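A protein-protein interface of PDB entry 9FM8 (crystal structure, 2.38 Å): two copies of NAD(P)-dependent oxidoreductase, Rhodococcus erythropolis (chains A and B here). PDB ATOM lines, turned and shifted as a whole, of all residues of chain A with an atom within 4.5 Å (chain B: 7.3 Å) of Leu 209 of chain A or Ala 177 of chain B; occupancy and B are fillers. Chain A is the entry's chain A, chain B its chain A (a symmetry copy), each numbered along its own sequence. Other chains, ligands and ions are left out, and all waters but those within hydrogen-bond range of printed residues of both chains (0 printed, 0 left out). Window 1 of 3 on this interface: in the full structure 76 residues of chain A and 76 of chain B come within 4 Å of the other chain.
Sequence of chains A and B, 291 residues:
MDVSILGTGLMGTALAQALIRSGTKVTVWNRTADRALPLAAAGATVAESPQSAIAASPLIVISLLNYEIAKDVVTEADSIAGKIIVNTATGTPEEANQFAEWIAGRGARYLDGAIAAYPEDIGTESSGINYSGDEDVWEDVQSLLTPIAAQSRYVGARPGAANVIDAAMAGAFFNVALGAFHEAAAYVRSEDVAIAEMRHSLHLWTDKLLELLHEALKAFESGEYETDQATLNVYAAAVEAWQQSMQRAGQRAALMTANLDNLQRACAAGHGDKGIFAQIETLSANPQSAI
Phe 173 of chain A touches Ala 180 of chain B (O to CB, 3.9 Å). Ala 177 of chain A touches Phe 173 of chain B (O to CE1, 3.9 Å). Lys 208 of chain A touches Phe 174 of chain B. CE2 of Phe 174 of chain B touches N of Leu 209 of chain A, at 3.5 Å. Leu 210 of chain A touches Leu 202 of chain B. CG2 of Thr 206 of chain B touches CD1 of Leu 210 of chain A, 3.6 Å away. Leu 212 of chain A touches Phe 174 of chain B (CD1 to CZ, 3.8 Å). Leu 178 of chain B touches Leu 212 of chain A (CD2 to CD1, 3.4 Å). Leu 213 of chain A touches Phe 181 of chain B (CD2 to CG, 3.5 Å). CG2 of Thr 206 of chain B touches CD1 of Leu 213 of chain A, at 3.95 Å.
A ring nitrogen (ND1) of His 182 of chain B lies within hydrogen-bond range of the backbone carbonyl oxygen (O) of Leu 178 of chain B.
Along chain B the printed residues that touch a printed residue of chain A span positions 173 to 209. Of the 11 printed residues of chain A, 8 touch a printed residue of chain B. Printed residues of chain A that touch a printed residue of chain B: Phe 173, Ala 177, Trp 205, Lys 208, Leu 209, Leu 210, Leu 212 and Leu 213. Hydrophobic or aromatic side chains of chain A that line the printed part of chain B: Phe 173, Ala 177, Trp 205, Leu 209, Leu 210, Leu 212 and Leu 213. Among the printed residues, no Asp or Glu carboxylate lies within 4 Å of a Lys or Arg side-chain nitrogen of the other chain.
Of the printed residues of chain B, Ala 177 of chain A touches Phe 173 (3.9 Å) and Leu 209 (3.9 Å). Leu 209 of chain A touches just these residues of chain B: Phe 174 (3.5 Å) and Ala 177 (3.9 Å). Printed residues of chain B within 4 Å of Leu 210 of chain A: Leu 202 and Thr 206. Gly 171 of chain B touches none of the printed residues of chain A. Of the printed residues of chain A, Phe 174 of chain B touches Trp 205 (3.4 Å), Lys 208 (3.8 Å), Leu 209 (3.5 Å) and Leu 212 (3.8 Å). Asn 175 of chain B touches none of the printed residues of chain A. Of the printed residues of chain A, Leu 209 of chain B touches Ala 177. The nearest residue of chain A that does not touch Ala 177 of chain B is Ala 177 of chain A (4.02 Å). The nearest printed residue of chain A that does not touch Phe 181 of chain B is Leu 212 of chain A (5.9 Å).
Phe 173 of chain A touches Ala 177 of chain B, and with the chains exchanged Ala 177 of chain A touches Phe 173 of chain B. Ala 177 of chain A touches Leu 209 of chain B, and with the chains exchanged Leu 209 of chain A touches Ala 177 of chain B.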
ATOM      1  N   PHE A 173     -15.423  21.368  18.390  1.00  0.00           N
ATOM      2  CA  PHE A 173     -16.274  22.004  19.383  1.00  0.00           C
ATOM      3  C   PHE A 173     -17.737  21.597  19.204  1.00  0.00           C
ATOM      4  O   PHE A 173     -18.247  20.816  19.986  1.00  0.00           O
ATOM      5  CB  PHE A 173     -16.129  23.529  19.344  1.00  0.00           C
ATOM      6  CG  PHE A 173     -17.219  24.200  20.162  1.00  0.00           C
ATOM      7  CD1 PHE A 173     -17.256  24.059  21.542  1.00  0.00           C
ATOM      8  CD2 PHE A 173     -18.235  24.921  19.542  1.00  0.00           C
ATOM      9  CE1 PHE A 173     -18.278  24.636  22.284  1.00  0.00           C
ATOM     10  CE2 PHE A 173     -19.254  25.500  20.275  1.00  0.00           C
ATOM     11  CZ  PHE A 173     -19.279  25.356  21.647  1.00  0.00           C
ATOM     12  N   ALA A 177     -19.842  18.898  21.432  1.00  0.00           N
ATOM     13  CA  ALA A 177     -20.774  19.522  22.355  1.00  0.00           C
ATOM     14  C   ALA A 177     -22.181  18.962  22.171  1.00  0.00           C
ATOM     15  O   ALA A 177     -22.880  18.727  23.140  1.00  0.00           O
ATOM     16  CB  ALA A 177     -20.752  21.021  22.156  1.00  0.00           C
ATOM     17  N   TRP A 205     -27.113  27.640  30.416  1.00  0.00           N
ATOM     18  CA  TRP A 205     -25.905  26.854  30.222  1.00  0.00           C
ATOM     19  C   TRP A 205     -25.145  27.261  28.961  1.00  0.00           C
ATOM     20  O   TRP A 205     -23.912  27.317  28.980  1.00  0.00           O
ATOM     21  CB  TRP A 205     -26.237  25.354  30.238  1.00  0.00           C
ATOM     22  CG  TRP A 205     -26.500  24.891  31.646  1.00  0.00           C
ATOM     23  CD1 TRP A 205     -27.690  24.537  32.193  1.00  0.00           C
ATOM     24  CD2 TRP A 205     -25.535  24.814  32.715  1.00  0.00           C
ATOM     25  NE1 TRP A 205     -27.525  24.214  33.511  1.00  0.00           N
ATOM     26  CE2 TRP A 205     -26.216  24.376  33.858  1.00  0.00           C
ATOM     27  CE3 TRP A 205     -24.165  25.063  32.808  1.00  0.00           C
ATOM     28  CZ2 TRP A 205     -25.577  24.177  35.075  1.00  0.00           C
ATOM     29  CZ3 TRP A 205     -23.531  24.875  34.010  1.00  0.00           C
ATOM     30  CH2 TRP A 205     -24.230  24.435  35.128  1.00  0.00           C
ATOM     31  N   THR A 206     -25.866  27.576  27.882  1.00  0.00           N
ATOM     32  CA  THR A 206     -25.204  27.995  26.656  1.00  0.00           C
ATOM     33  C   THR A 206     -24.656  29.417  26.831  1.00  0.00           C
ATOM     34  O   THR A 206     -23.525  29.703  26.433  1.00  0.00           O
ATOM     35  CB  THR A 206     -26.156  27.842  25.468  1.00  0.00           C
ATOM     36  OG1 THR A 206     -27.193  28.807  25.602  1.00  0.00           O
ATOM     37  CG2 THR A 206     -26.747  26.443  25.363  1.00  0.00           C
ATOM     38  N   ASP A 207     -25.439  30.286  27.484  1.00  0.00           N
ATOM     39  CA  ASP A 207     -24.975  31.597  27.925  1.00  0.00           C
ATOM     40  C   ASP A 207     -23.719  31.500  28.795  1.00  0.00           C
ATOM     41  O   ASP A 207     -22.800  32.299  28.625  1.00  0.00           O
ATOM     42  CB  ASP A 207     -26.062  32.355  28.669  1.00  0.00           C
ATOM     43  CG  ASP A 207     -27.116  33.006  27.788  1.00  0.00           C
ATOM     44  OD1 ASP A 207     -26.845  33.185  26.585  1.00  0.00           O
ATOM     45  OD2 ASP A 207     -28.206  33.316  28.308  1.00  0.00           O
ATOM     46  N   LYS A 208     -23.682  30.541  29.730  1.00  0.00           N
ATOM     47  CA  LYS A 208     -22.514  30.356  30.583  1.00  0.00           C
ATOM     48  C   LYS A 208     -21.327  29.854  29.754  1.00  0.00           C
ATOM     49  O   LYS A 208     -20.201  30.318  29.934  1.00  0.00           O
ATOM     50  CB  LYS A 208     -22.803  29.421  31.765  1.00  0.00           C
ATOM     51  CG  LYS A 208     -21.953  29.657  33.034  1.00  0.00           C
ATOM     52  N   LEU A 209     -21.586  28.912  28.839  1.00  0.00           N
ATOM     53  CA  LEU A 209     -20.524  28.303  28.054  1.00  0.00           C
ATOM     54  C   LEU A 209     -19.817  29.370  27.221  1.00  0.00           C
ATOM     55  O   LEU A 209     -18.587  29.342  27.100  1.00  0.00           O
ATOM     56  CB  LEU A 209     -21.104  27.200  27.176  1.00  0.00           C
ATOM     57  CG  LEU A 209     -20.113  26.484  26.258  1.00  0.00           C
ATOM     58  CD1 LEU A 209     -18.971  25.808  26.997  1.00  0.00           C
ATOM     59  CD2 LEU A 209     -20.895  25.475  25.480  1.00  0.00           C
ATOM     60  N   LEU A 210     -20.607  30.314  26.676  1.00  0.00           N
ATOM     61  CA  LEU A 210     -20.083  31.350  25.794  1.00  0.00           C
ATOM     62  C   LEU A 210     -19.048  32.199  26.527  1.00  0.00           C
ATOM     63  O   LEU A 210     -17.933  32.363  26.030  1.00  0.00           O
ATOM     64  CB  LEU A 210     -21.201  32.223  25.233  1.00  0.00           C
ATOM     65  CG  LEU A 210     -20.755  33.356  24.299  1.00  0.00           C
ATOM     66  CD1 LEU A 210     -20.163  32.826  23.010  1.00  0.00           C
ATOM     67  CD2 LEU A 210     -21.915  34.287  24.002  1.00  0.00           C
ATOM     68  N   GLU A 211     -19.447  32.719  27.703  1.00  0.00           N
ATOM     69  CA  GLU A 211     -18.573  33.476  28.589  1.00  0.00           C
ATOM     70  C   GLU A 211     -17.261  32.725  28.786  1.00  0.00           C
ATOM     71  O   GLU A 211     -16.181  33.291  28.592  1.00  0.00           O
ATOM     72  CB  GLU A 211     -19.184  33.654  29.978  1.00  0.00           C
ATOM     73  CG  GLU A 211     -19.915  34.974  30.210  1.00  0.00           C
ATOM     74  CD  GLU A 211     -20.283  35.171  31.677  1.00  0.00           C
ATOM     75  OE1 GLU A 211     -19.355  35.121  32.531  1.00  0.00           O
ATOM     76  OE2 GLU A 211     -21.492  35.361  31.967  1.00  0.00           O
ATOM     77  N   LEU A 212     -17.378  31.445  29.172  1.00  0.00           N
ATOM     78  CA  LEU A 212     -16.205  30.660  29.505  1.00  0.00           C
ATOM     79  C   LEU A 212     -15.319  30.489  28.280  1.00  0.00           C
ATOM     80  O   LEU A 212     -14.088  30.578  28.390  1.00  0.00           O
ATOM     81  CB  LEU A 212     -16.568  29.314  30.116  1.00  0.00           C
ATOM     82  CG  LEU A 212     -16.516  29.255  31.644  1.00  0.00           C
ATOM     83  CD1 LEU A 212     -16.049  27.872  32.028  1.00  0.00           C
ATOM     84  CD2 LEU A 212     -15.605  30.292  32.278  1.00  0.00           C
ATOM     85  N   LEU A 213     -15.965  30.278  27.123  1.00  0.00           N
ATOM     86  CA  LEU A 213     -15.235  30.172  25.876  1.00  0.00           C
ATOM     87  C   LEU A 213     -14.377  31.423  25.696  1.00  0.00           C
ATOM     88  O   LEU A 213     -13.175  31.325  25.447  1.00  0.00           O
ATOM     89  CB  LEU A 213     -16.187  29.965  24.700  1.00  0.00           C
ATOM     90  CG  LEU A 213     -16.966  28.645  24.655  1.00  0.00           C
ATOM     91  CD1 LEU A 213     -17.595  28.477  23.264  1.00  0.00           C
ATOM     92  CD2 LEU A 213     -16.129  27.429  25.030  1.00  0.00           C
ATOM     93  N   TYR B 118     -23.035  31.208  39.258  1.00  0.00           N
ATOM     94  CA  TYR B 118     -21.944  31.727  40.058  1.00  0.00           C
ATOM     95  C   TYR B 118     -22.555  32.576  41.175  1.00  0.00           C
ATOM     96  O   TYR B 118     -23.608  33.198  40.982  1.00  0.00           O
ATOM     97  CB  TYR B 118     -20.983  32.458  39.110  1.00  0.00           C
ATOM     98  CG  TYR B 118     -20.300  31.583  38.061  1.00  0.00           C
ATOM     99  CD1 TYR B 118     -19.997  30.247  38.325  1.00  0.00           C
ATOM    100  CD2 TYR B 118     -19.941  32.094  36.815  1.00  0.00           C
ATOM    101  CE1 TYR B 118     -19.374  29.444  37.384  1.00  0.00           C
ATOM    102  CE2 TYR B 118     -19.322  31.299  35.860  1.00  0.00           C
ATOM    103  CZ  TYR B 118     -19.035  29.971  36.148  1.00  0.00           C
ATOM    104  OH  TYR B 118     -18.416  29.149  35.246  1.00  0.00           O
ATOM    105  N   GLY B 171     -21.837  18.617  34.042  1.00  0.00           N
ATOM    106  CA  GLY B 171     -20.760  17.653  33.853  1.00  0.00           C
ATOM    107  C   GLY B 171     -20.769  17.057  32.448  1.00  0.00           C
ATOM    108  O   GLY B 171     -19.898  17.376  31.638  1.00  0.00           O
ATOM    109  N   ALA B 172     -21.771  16.199  32.209  1.00  0.00           N
ATOM    110  CA  ALA B 172     -21.976  15.492  30.954  1.00  0.00           C
ATOM    111  C   ALA B 172     -21.942  16.437  29.755  1.00  0.00           C
ATOM    112  O   ALA B 172     -21.247  16.162  28.771  1.00  0.00           O
ATOM    113  CB  ALA B 172     -23.295  14.757  31.011  1.00  0.00           C
ATOM    114  N   PHE B 173     -22.722  17.523  29.853  1.00  0.00           N
ATOM    115  CA  PHE B 173     -22.822  18.526  28.804  1.00  0.00           C
ATOM    116  C   PHE B 173     -21.747  19.602  28.961  1.00  0.00           C
ATOM    117  O   PHE B 173     -20.793  19.617  28.204  1.00  0.00           O
ATOM    118  CB  PHE B 173     -24.217  19.158  28.770  1.00  0.00           C
ATOM    119  CG  PHE B 173     -24.233  20.394  27.887  1.00  0.00           C
ATOM    120  CD1 PHE B 173     -24.052  20.286  26.516  1.00  0.00           C
ATOM    121  CD2 PHE B 173     -24.372  21.663  28.440  1.00  0.00           C
ATOM    122  CE1 PHE B 173     -24.023  21.421  25.716  1.00  0.00           C
ATOM    123  CE2 PHE B 173     -24.346  22.797  27.650  1.00  0.00           C
ATOM    124  CZ  PHE B 173     -24.168  22.678  26.287  1.00  0.00           C
ATOM    125  N   PHE B 174     -21.897  20.475  29.960  1.00  0.00           N
ATOM    126  CA  PHE B 174     -21.160  21.730  30.058  1.00  0.00           C
ATOM    127  C   PHE B 174     -19.650  21.507  30.045  1.00  0.00           C
ATOM    128  O   PHE B 174     -18.932  22.147  29.285  1.00  0.00           O
ATOM    129  CB  PHE B 174     -21.528  22.521  31.325  1.00  0.00           C
ATOM    130  CG  PHE B 174     -20.814  23.865  31.410  1.00  0.00           C
ATOM    131  CD1 PHE B 174     -19.557  23.973  31.991  1.00  0.00           C
ATOM    132  CD2 PHE B 174     -21.369  25.005  30.834  1.00  0.00           C
ATOM    133  CE1 PHE B 174     -18.880  25.193  31.999  1.00  0.00           C
ATOM    134  CE2 PHE B 174     -20.704  26.226  30.868  1.00  0.00           C
ATOM    135  CZ  PHE B 174     -19.458  26.322  31.446  1.00  0.00           C
ATOM    136  N   ASN B 175     -19.163  20.637  30.925  1.00  0.00           N
ATOM    137  CA  ASN B 175     -17.734  20.518  31.136  1.00  0.00           C
ATOM    138  C   ASN B 175     -17.059  19.907  29.918  1.00  0.00           C
ATOM    139  O   ASN B 175     -15.955  20.305  29.556  1.00  0.00           O
ATOM    140  CB  ASN B 175     -17.417  19.648  32.341  1.00  0.00           C
ATOM    141  CG  ASN B 175     -16.187  20.159  33.043  1.00  0.00           C
ATOM    142  OD1 ASN B 175     -16.297  21.031  33.913  1.00  0.00           O
ATOM    143  ND2 ASN B 175     -15.024  19.645  32.674  1.00  0.00           N
ATOM    144  N   VAL B 176     -17.720  18.899  29.347  1.00  0.00           N
ATOM    145  CA  VAL B 176     -17.263  18.235  28.140  1.00  0.00           C
ATOM    146  C   VAL B 176     -17.211  19.229  26.977  1.00  0.00           C
ATOM    147  O   VAL B 176     -16.222  19.328  26.248  1.00  0.00           O
ATOM    148  CB  VAL B 176     -18.211  17.068  27.827  1.00  0.00           C
ATOM    149  CG1 VAL B 176     -17.905  16.467  26.469  1.00  0.00           C
ATOM    150  CG2 VAL B 176     -18.171  15.993  28.905  1.00  0.00           C
ATOM    151  N   ALA B 177     -18.294  19.977  26.811  1.00  0.00           N
ATOM    152  CA  ALA B 177     -18.345  21.048  25.831  1.00  0.00           C
ATOM    153  C   ALA B 177     -17.166  22.000  26.002  1.00  0.00           C
ATOM    154  O   ALA B 177     -16.586  22.441  25.025  1.00  0.00           O
ATOM    155  CB  ALA B 177     -19.662  21.782  25.954  1.00  0.00           C
ATOM    156  N   LEU B 178     -16.821  22.347  27.239  1.00  0.00           N
ATOM    157  CA  LEU B 178     -15.731  23.276  27.492  1.00  0.00           C
ATOM    158  C   LEU B 178     -14.393  22.623  27.141  1.00  0.00           C
ATOM    159  O   LEU B 178     -13.427  23.307  26.817  1.00  0.00           O
ATOM    160  CB  LEU B 178     -15.762  23.730  28.950  1.00  0.00           C
ATOM    161  CG  LEU B 178     -14.584  24.598  29.409  1.00  0.00           C
ATOM    162  CD1 LEU B 178     -14.407  25.847  28.551  1.00  0.00           C
ATOM    163  CD2 LEU B 178     -14.785  24.981  30.860  1.00  0.00           C
ATOM    164  N   GLY B 179     -14.326  21.297  27.222  1.00  0.00           N
ATOM    165  CA  GLY B 179     -13.117  20.601  26.813  1.00  0.00           C
ATOM    166  C   GLY B 179     -13.004  20.540  25.296  1.00  0.00           C
ATOM    167  O   GLY B 179     -11.946  20.791  24.724  1.00  0.00           O
ATOM    168  N   ALA B 180     -14.128  20.211  24.661  1.00  0.00           N
ATOM    169  CA  ALA B 180     -14.223  20.153  23.216  1.00  0.00           C
ATOM    170  C   ALA B 180     -13.588  21.391  22.599  1.00  0.00           C
ATOM    171  O   ALA B 180     -12.877  21.291  21.605  1.00  0.00           O
ATOM    172  CB  ALA B 180     -15.665  20.028  22.825  1.00  0.00           C
ATOM    173  N   PHE B 181     -13.836  22.549  23.219  1.00  0.00           N
ATOM    174  CA  PHE B 181     -13.330  23.819  22.729  1.00  0.00           C
ATOM    175  C   PHE B 181     -11.824  23.935  22.941  1.00  0.00           C
ATOM    176  O   PHE B 181     -11.165  24.728  22.283  1.00  0.00           O
ATOM    177  CB  PHE B 181     -14.047  24.968  23.441  1.00  0.00           C
ATOM    178  CG  PHE B 181     -13.597  26.325  22.933  1.00  0.00           C
ATOM    179  CD1 PHE B 181     -13.999  26.786  21.690  1.00  0.00           C
ATOM    180  CD2 PHE B 181     -12.787  27.140  23.705  1.00  0.00           C
ATOM    181  CE1 PHE B 181     -13.574  28.017  21.218  1.00  0.00           C
ATOM    182  CE2 PHE B 181     -12.371  28.376  23.233  1.00  0.00           C
ATOM    183  CZ  PHE B 181     -12.756  28.804  21.990  1.00  0.00           C
ATOM    184  N   HIS B 182     -11.302  23.186  23.909  1.00  0.00           N
ATOM    185  CA  HIS B 182      -9.871  23.142  24.142  1.00  0.00           C
ATOM    186  C   HIS B 182      -9.262  22.357  22.987  1.00  0.00           C
ATOM    187  O   HIS B 182      -8.313  22.815  22.363  1.00  0.00           O
ATOM    188  CB  HIS B 182      -9.549  22.574  25.539  1.00  0.00           C
ATOM    189  CG  HIS B 182      -9.774  23.499  26.700  1.00  0.00           C
ATOM    190  ND1 HIS B 182     -11.020  23.941  27.102  1.00  0.00           N
ATOM    191  CD2 HIS B 182      -8.894  24.066  27.539  1.00  0.00           C
ATOM    192  CE1 HIS B 182     -10.884  24.751  28.141  1.00  0.00           C
ATOM    193  NE2 HIS B 182      -9.600  24.847  28.417  1.00  0.00           N
ATOM    194  N   GLU B 183      -9.827  21.179  22.695  1.00  0.00           N
ATOM    195  CA  GLU B 183      -9.394  20.398  21.546  1.00  0.00           C
ATOM    196  C   GLU B 183      -9.427  21.277  20.301  1.00  0.00           C
ATOM    197  O   GLU B 183      -8.470  21.332  19.538  1.00  0.00           O
ATOM    198  CB  GLU B 183     -10.253  19.156  21.349  1.00  0.00           C
ATOM    199  CG  GLU B 183     -10.096  18.151  22.487  1.00  0.00           C
ATOM    200  CD  GLU B 183     -10.632  16.763  22.170  1.00  0.00           C
ATOM    201  OE1 GLU B 183     -11.364  16.591  21.157  1.00  0.00           O
ATOM    202  OE2 GLU B 183     -10.300  15.840  22.945  1.00  0.00           O
ATOM    203  N   LEU B 202     -17.869  32.829  18.122  1.00  0.00           N
ATOM    204  CA  LEU B 202     -18.263  32.116  19.325  1.00  0.00           C
ATOM    205  C   LEU B 202     -19.783  32.165  19.543  1.00  0.00           C
ATOM    206  O   LEU B 202     -20.433  31.128  19.645  1.00  0.00           O
ATOM    207  CB  LEU B 202     -17.439  32.664  20.491  1.00  0.00           C
ATOM    208  CG  LEU B 202     -16.299  31.783  21.023  1.00  0.00           C
ATOM    209  CD1 LEU B 202     -15.599  30.878  20.025  1.00  0.00           C
ATOM    210  CD2 LEU B 202     -15.251  32.673  21.671  1.00  0.00           C
ATOM    211  N   THR B 206     -22.636  29.174  19.757  1.00  0.00           N
ATOM    212  CA  THR B 206     -23.364  28.870  20.979  1.00  0.00           C
ATOM    213  C   THR B 206     -24.865  29.090  20.748  1.00  0.00           C
ATOM    214  O   THR B 206     -25.686  28.272  21.164  1.00  0.00           O
ATOM    215  CB  THR B 206     -22.793  29.680  22.144  1.00  0.00           C
ATOM    216  OG1 THR B 206     -23.111  31.051  21.932  1.00  0.00           O
ATOM    217  CG2 THR B 206     -21.290  29.504  22.302  1.00  0.00           C
ATOM    218  N   LEU B 209     -25.894  26.076  18.860  1.00  0.00           N
ATOM    219  CA  LEU B 209     -25.917  24.893  19.705  1.00  0.00           C
ATOM    220  C   LEU B 209     -27.218  24.851  20.503  1.00  0.00           C
ATOM    221  O   LEU B 209     -27.809  23.776  20.661  1.00  0.00           O
ATOM    222  CB  LEU B 209     -24.698  24.895  20.620  1.00  0.00           C
ATOM    223  CG  LEU B 209     -24.596  23.726  21.602  1.00  0.00           C
ATOM    224  CD1 LEU B 209     -24.556  22.364  20.932  1.00  0.00           C
ATOM    225  CD2 LEU B 209     -23.356  23.944  22.407  1.00  0.00           C
ATOM    226  N   LEU B 255     -11.756  13.596  22.610  1.00  0.00           N
ATOM    227  CA  LEU B 255     -13.173  13.934  22.610  1.00  0.00           C
ATOM    228  C   LEU B 255     -13.763  13.632  21.235  1.00  0.00           C
ATOM    229  O   LEU B 255     -14.870  13.089  21.144  1.00  0.00           O
ATOM    230  CB  LEU B 255     -13.431  15.384  23.018  1.00  0.00           C
ATOM    231  CG  LEU B 255     -13.147  15.726  24.483  1.00  0.00           C
ATOM    232  CD1 LEU B 255     -13.049  17.227  24.763  1.00  0.00           C
ATOM    233  CD2 LEU B 255     -14.237  15.104  25.342  1.00  0.00           C
